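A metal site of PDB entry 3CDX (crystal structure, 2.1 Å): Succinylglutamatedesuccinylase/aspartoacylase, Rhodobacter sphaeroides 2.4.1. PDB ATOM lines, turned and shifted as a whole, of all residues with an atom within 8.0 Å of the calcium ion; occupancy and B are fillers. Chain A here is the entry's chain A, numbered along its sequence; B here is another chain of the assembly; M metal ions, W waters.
NH1 of Arg 105 touches the calcium ion (3.96 Å).
Thr 150 touches the calcium ion (O to CA, 3.8 Å).
Water W1 bridges OE2 of Glu 214 and O of Thr 150.
The side-chain carboxylate of Glu 66 lies close to the backbone NH of Thr 150, 3.2 Å away.
The side-chain carboxylate of Glu 66 lies close to the guanidinium group of Arg 105 (3.4 Å).
The backbone NH (N) of His 149 sits at hydrogen-bond distance from the side-chain hydroxyl (OG1) of Thr 213 (3.0 Å).
NE2 of His 149 lies within hydrogen-bond range of OD2 of Asp 147, at 2.6 Å.
A ring nitrogen (NE2) of His 63 sits at hydrogen-bond distance from the side-chain carboxylate (OD1) of Asp 113 (2.7 Å).
N of Thr 150 sits close to OE1 of Glu 214 (3.4 Å).
The side-chain hydroxyl of Thr 150 sits at hydrogen-bond distance from the backbone NH of Gly 152, at 3.1 Å.
The guanidinium group (NE) of Arg 105 is in salt-bridge range of the side-chain carboxylate (OD2) of Asp 113 (3.1 Å).
The calcium ion is bound by OE1 of Glu 66 (2.3 Å), ND1 of His 149 (2.3 Å), ND1 of His 63 (2.4 Å) and OE2 of Glu 66 (2.4 Å).
Slightly farther from the calcium ion lies water W1 (2.9 Å).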
ATOM      1  N   GLY A  61      -4.520   2.459 -13.453  1.00  0.00           N
ATOM      2  CA  GLY A  61      -4.685   3.479 -12.407  1.00  0.00           C
ATOM      3  C   GLY A  61      -6.085   4.076 -12.372  1.00  0.00           C
ATOM      4  O   GLY A  61      -6.274   5.203 -11.930  1.00  0.00           O
ATOM      5  N   VAL A  62      -7.069   3.297 -12.833  1.00  0.00           N
ATOM      6  CA  VAL A  62      -8.462   3.699 -12.679  1.00  0.00           C
ATOM      7  C   VAL A  62      -8.772   3.813 -11.187  1.00  0.00           C
ATOM      8  O   VAL A  62      -9.540   4.684 -10.776  1.00  0.00           O
ATOM      9  CB  VAL A  62      -9.394   2.705 -13.422  1.00  0.00           C
ATOM     10  CG1 VAL A  62     -10.844   2.760 -12.891  1.00  0.00           C
ATOM     11  CG2 VAL A  62      -9.341   3.013 -14.942  1.00  0.00           C
ATOM     12  N   HIS A  63      -8.146   2.926 -10.404  1.00  0.00           N
ATOM     13  CA  HIS A  63      -8.081   3.045  -8.956  1.00  0.00           C
ATOM     14  C   HIS A  63      -6.657   3.428  -8.573  1.00  0.00           C
ATOM     15  O   HIS A  63      -5.697   2.863  -9.103  1.00  0.00           O
ATOM     16  CB  HIS A  63      -8.520   1.733  -8.274  1.00  0.00           C
ATOM     17  CG  HIS A  63      -9.995   1.476  -8.405  1.00  0.00           C
ATOM     18  ND1 HIS A  63     -10.516   0.245  -8.753  1.00  0.00           N
ATOM     19  CD2 HIS A  63     -11.064   2.297  -8.275  1.00  0.00           C
ATOM     20  CE1 HIS A  63     -11.834   0.320  -8.830  1.00  0.00           C
ATOM     21  NE2 HIS A  63     -12.196   1.548  -8.530  1.00  0.00           N
ATOM     22  N   GLY A  64      -6.524   4.432  -7.727  1.00  0.00           N
ATOM     23  CA  GLY A  64      -5.218   5.002  -7.446  1.00  0.00           C
ATOM     24  C   GLY A  64      -4.232   4.044  -6.776  1.00  0.00           C
ATOM     25  O   GLY A  64      -3.006   4.219  -6.939  1.00  0.00           O
ATOM     26  N   ASP A  65      -4.764   3.065  -6.045  1.00  0.00           N
ATOM     27  CA  ASP A  65      -3.937   2.110  -5.286  1.00  0.00           C
ATOM     28  C   ASP A  65      -3.685   0.778  -6.030  1.00  0.00           C
ATOM     29  O   ASP A  65      -3.269  -0.205  -5.434  1.00  0.00           O
ATOM     30  CB  ASP A  65      -4.562   1.819  -3.898  1.00  0.00           C
ATOM     31  CG  ASP A  65      -5.969   1.217  -3.975  1.00  0.00           C
ATOM     32  OD1 ASP A  65      -6.629   1.242  -5.039  1.00  0.00           O
ATOM     33  OD2 ASP A  65      -6.438   0.748  -2.929  1.00  0.00           O
ATOM     34  N   GLU A  66      -3.958   0.743  -7.325  1.00  0.00           N
ATOM     35  CA  GLU A  66      -3.722  -0.478  -8.076  1.00  0.00           C
ATOM     36  C   GLU A  66      -2.588  -0.198  -9.027  1.00  0.00           C
ATOM     37  O   GLU A  66      -2.801   0.437 -10.033  1.00  0.00           O
ATOM     38  CB  GLU A  66      -4.996  -0.899  -8.765  1.00  0.00           C
ATOM     39  CG  GLU A  66      -6.034  -1.204  -7.748  1.00  0.00           C
ATOM     40  CD  GLU A  66      -7.393  -1.485  -8.319  1.00  0.00           C
ATOM     41  OE1 GLU A  66      -7.492  -1.648  -9.573  1.00  0.00           O
ATOM     42  OE2 GLU A  66      -8.343  -1.508  -7.497  1.00  0.00           O
ATOM     43  N   ARG A 105      -8.322   3.952  -3.464  1.00  0.00           N
ATOM     44  CA  ARG A 105      -9.334   3.467  -4.404  1.00  0.00           C
ATOM     45  C   ARG A 105     -10.308   4.567  -4.768  1.00  0.00           C
ATOM     46  O   ARG A 105     -10.565   4.779  -5.962  1.00  0.00           O
ATOM     47  CB  ARG A 105     -10.101   2.310  -3.774  1.00  0.00           C
ATOM     48  CG  ARG A 105     -11.002   1.601  -4.757  1.00  0.00           C
ATOM     49  CD  ARG A 105     -11.784   0.492  -4.028  1.00  0.00           C
ATOM     50  NE  ARG A 105     -12.777  -0.116  -4.902  1.00  0.00           N
ATOM     51  CZ  ARG A 105     -12.526  -1.125  -5.726  1.00  0.00           C
ATOM     52  NH1 ARG A 105     -11.302  -1.643  -5.803  1.00  0.00           N
ATOM     53  NH2 ARG A 105     -13.492  -1.617  -6.479  1.00  0.00           N
ATOM     54  N   ASP A 113     -16.009   6.230  -5.975  1.00  0.00           N
ATOM     55  CA  ASP A 113     -15.335   5.140  -6.650  1.00  0.00           C
ATOM     56  C   ASP A 113     -15.631   5.351  -8.123  1.00  0.00           C
ATOM     57  O   ASP A 113     -16.758   5.157  -8.561  1.00  0.00           O
ATOM     58  CB  ASP A 113     -15.901   3.799  -6.198  1.00  0.00           C
ATOM     59  CG  ASP A 113     -15.113   2.621  -6.763  1.00  0.00           C
ATOM     60  OD1 ASP A 113     -14.561   2.728  -7.887  1.00  0.00           O
ATOM     61  OD2 ASP A 113     -15.049   1.578  -6.055  1.00  0.00           O
ATOM     62  N   ASN A 115     -15.167   3.726 -10.644  1.00  0.00           N
ATOM     63  CA  ASN A 115     -15.639   2.532 -11.321  1.00  0.00           C
ATOM     64  C   ASN A 115     -17.026   2.115 -10.860  1.00  0.00           C
ATOM     65  O   ASN A 115     -17.459   0.988 -11.105  1.00  0.00           O
ATOM     66  CB  ASN A 115     -14.653   1.386 -11.127  1.00  0.00           C
ATOM     67  CG  ASN A 115     -14.295   0.674 -12.429  1.00  0.00           C
ATOM     68  OD1 ASN A 115     -14.505   1.202 -13.516  1.00  0.00           O
ATOM     69  ND2 ASN A 115     -13.694  -0.534 -12.309  1.00  0.00           N
ATOM     70  N   ARG A 116     -17.704   2.994 -10.132  1.00  0.00           N
ATOM     71  CA  ARG A 116     -19.141   2.887  -9.938  1.00  0.00           C
ATOM     72  C   ARG A 116     -19.808   4.113 -10.600  1.00  0.00           C
ATOM     73  O   ARG A 116     -20.985   4.373 -10.313  1.00  0.00           O
ATOM     74  CB  ARG A 116     -19.495   2.832  -8.435  1.00  0.00           C
ATOM     75  CG  ARG A 116     -18.856   1.713  -7.625  1.00  0.00           C
ATOM     76  CD  ARG A 116     -19.179   0.330  -8.209  1.00  0.00           C
ATOM     77  NE  ARG A 116     -18.665  -0.793  -7.420  1.00  0.00           N
ATOM     78  CZ  ARG A 116     -17.626  -1.557  -7.747  1.00  0.00           C
ATOM     79  NH1 ARG A 116     -16.935  -1.335  -8.853  1.00  0.00           N
ATOM     80  NH2 ARG A 116     -17.253  -2.554  -6.937  1.00  0.00           N
ATOM     81  N   ASP A 147      -7.952  -3.274 -19.349  1.00  0.00           N
ATOM     82  CA  ASP A 147      -8.048  -2.389 -18.201  1.00  0.00           C
ATOM     83  C   ASP A 147      -7.363  -3.089 -17.030  1.00  0.00           C
ATOM     84  O   ASP A 147      -7.806  -4.144 -16.552  1.00  0.00           O
ATOM     85  CB  ASP A 147      -9.540  -1.985 -17.963  1.00  0.00           C
ATOM     86  CG  ASP A 147      -9.705  -0.926 -16.866  1.00  0.00           C
ATOM     87  OD1 ASP A 147      -8.789  -0.078 -16.624  1.00  0.00           O
ATOM     88  OD2 ASP A 147     -10.767  -1.001 -16.200  1.00  0.00           O
ATOM     89  N   MET A 148      -6.229  -2.534 -16.628  1.00  0.00           N
ATOM     90  CA  MET A 148      -5.391  -3.205 -15.639  1.00  0.00           C
ATOM     91  C   MET A 148      -5.687  -2.822 -14.154  1.00  0.00           C
ATOM     92  O   MET A 148      -5.516  -1.659 -13.708  1.00  0.00           O
ATOM     93  CB  MET A 148      -3.909  -2.945 -15.980  1.00  0.00           C
ATOM     94  CG  MET A 148      -3.487  -3.415 -17.424  1.00  0.00           C
ATOM     95  SD  MET A 148      -1.729  -3.344 -17.873  1.00  0.00           S
ATOM     96  CE  MET A 148      -1.069  -4.774 -17.058  1.00  0.00           C
ATOM     97  N   HIS A 149      -6.089  -3.836 -13.395  1.00  0.00           N
ATOM     98  CA  HIS A 149      -6.478  -3.687 -12.016  1.00  0.00           C
ATOM     99  C   HIS A 149      -5.688  -4.633 -11.120  1.00  0.00           C
ATOM    100  O   HIS A 149      -4.973  -5.541 -11.606  1.00  0.00           O
ATOM    101  CB  HIS A 149      -7.993  -3.960 -11.875  1.00  0.00           C
ATOM    102  CG  HIS A 149      -8.849  -2.878 -12.471  1.00  0.00           C
ATOM    103  ND1 HIS A 149      -9.404  -1.865 -11.713  1.00  0.00           N
ATOM    104  CD2 HIS A 149      -9.205  -2.630 -13.753  1.00  0.00           C
ATOM    105  CE1 HIS A 149     -10.069  -1.046 -12.497  1.00  0.00           C
ATOM    106  NE2 HIS A 149      -9.982  -1.498 -13.739  1.00  0.00           N
ATOM    107  N   THR A 150      -5.832  -4.412  -9.813  1.00  0.00           N
ATOM    108  CA  THR A 150      -5.418  -5.327  -8.757  1.00  0.00           C
ATOM    109  C   THR A 150      -6.463  -5.164  -7.661  1.00  0.00           C
ATOM    110  O   THR A 150      -7.391  -4.351  -7.815  1.00  0.00           O
ATOM    111  CB  THR A 150      -4.033  -4.989  -8.152  1.00  0.00           C
ATOM    112  OG1 THR A 150      -4.146  -3.804  -7.330  1.00  0.00           O
ATOM    113  CG2 THR A 150      -2.961  -4.763  -9.222  1.00  0.00           C
ATOM    114  N   ALA A 151      -6.301  -5.890  -6.550  1.00  0.00           N
ATOM    115  CA  ALA A 151      -7.263  -5.760  -5.440  1.00  0.00           C
ATOM    116  C   ALA A 151      -6.973  -4.586  -4.501  1.00  0.00           C
ATOM    117  O   ALA A 151      -7.690  -4.402  -3.513  1.00  0.00           O
ATOM    118  CB  ALA A 151      -7.371  -7.058  -4.673  1.00  0.00           C
ATOM    119  N   GLY A 152      -5.936  -3.798  -4.827  1.00  0.00           N
ATOM    120  CA  GLY A 152      -5.589  -2.580  -4.085  1.00  0.00           C
ATOM    121  C   GLY A 152      -5.294  -2.890  -2.629  1.00  0.00           C
ATOM    122  O   GLY A 152      -4.490  -3.782  -2.317  1.00  0.00           O
ATOM    123  N   THR A 213      -7.633  -7.190 -15.614  1.00  0.00           N
ATOM    124  CA  THR A 213      -6.617  -7.941 -14.855  1.00  0.00           C
ATOM    125  C   THR A 213      -6.801  -7.834 -13.342  1.00  0.00           C
ATOM    126  O   THR A 213      -7.451  -6.899 -12.852  1.00  0.00           O
ATOM    127  CB  THR A 213      -5.177  -7.540 -15.207  1.00  0.00           C
ATOM    128  OG1 THR A 213      -4.833  -6.309 -14.573  1.00  0.00           O
ATOM    129  CG2 THR A 213      -4.996  -7.387 -16.716  1.00  0.00           C
ATOM    130  N   GLU A 214      -6.336  -8.873 -12.624  1.00  0.00           N
ATOM    131  CA  GLU A 214      -6.110  -8.789 -11.208  1.00  0.00           C
ATOM    132  C   GLU A 214      -4.678  -9.273 -10.976  1.00  0.00           C
ATOM    133  O   GLU A 214      -4.375 -10.475 -11.049  1.00  0.00           O
ATOM    134  CB  GLU A 214      -7.159  -9.588 -10.432  1.00  0.00           C
ATOM    135  CG  GLU A 214      -8.643  -9.055 -10.513  1.00  0.00           C
ATOM    136  CD  GLU A 214      -8.831  -7.599 -10.029  1.00  0.00           C
ATOM    137  OE1 GLU A 214      -7.949  -7.062  -9.325  1.00  0.00           O
ATOM    138  OE2 GLU A 214      -9.877  -6.987 -10.344  1.00  0.00           O
ATOM    139  N   PHE A 320      -9.194 -14.378  -4.872  1.00  0.00           N
ATOM    140  CA  PHE A 320      -9.034 -13.247  -3.941  1.00  0.00           C
ATOM    141  C   PHE A 320      -8.927 -13.769  -2.535  1.00  0.00           C
ATOM    142  O   PHE A 320      -9.753 -14.578  -2.101  1.00  0.00           O
ATOM    143  CB  PHE A 320     -10.224 -12.277  -3.986  1.00  0.00           C
ATOM    144  CG  PHE A 320     -10.191 -11.287  -5.123  1.00  0.00           C
ATOM    145  CD1 PHE A 320      -9.669 -11.636  -6.361  1.00  0.00           C
ATOM    146  CD2 PHE A 320     -10.706  -9.989  -4.955  1.00  0.00           C
ATOM    147  CE1 PHE A 320      -9.629 -10.699  -7.419  1.00  0.00           C
ATOM    148  CE2 PHE A 320     -10.652  -9.043  -6.010  1.00  0.00           C
ATOM    149  CZ  PHE A 320     -10.125  -9.422  -7.241  1.00  0.00           C
ATOM    150  N   TRP B  38     -15.502  -4.145  -2.435  1.00  0.00           N
ATOM    151  CA  TRP B  38     -16.613  -5.065  -2.690  1.00  0.00           C
ATOM    152  C   TRP B  38     -17.392  -5.308  -1.399  1.00  0.00           C
ATOM    153  O   TRP B  38     -17.993  -6.358  -1.262  1.00  0.00           O
ATOM    154  CB  TRP B  38     -16.097  -6.413  -3.217  1.00  0.00           C
ATOM    155  CG  TRP B  38     -15.616  -6.434  -4.679  1.00  0.00           C
ATOM    156  CD1 TRP B  38     -15.287  -5.356  -5.456  1.00  0.00           C
ATOM    157  CD2 TRP B  38     -15.396  -7.593  -5.489  1.00  0.00           C
ATOM    158  NE1 TRP B  38     -14.882  -5.770  -6.701  1.00  0.00           N
ATOM    159  CE2 TRP B  38     -14.941  -7.138  -6.759  1.00  0.00           C
ATOM    160  CE3 TRP B  38     -15.528  -8.985  -5.288  1.00  0.00           C
ATOM    161  CZ2 TRP B  38     -14.626  -8.024  -7.806  1.00  0.00           C
ATOM    162  CZ3 TRP B  38     -15.226  -9.850  -6.337  1.00  0.00           C
ATOM    163  CH2 TRP B  38     -14.774  -9.365  -7.578  1.00  0.00           C
HETATM  164 CA    CA M   1      -9.730  -1.892  -9.430  1.00  0.00          CA
HETATM  165  O   HOH W   1      -9.918  -4.741  -8.901  1.00  0.00           O
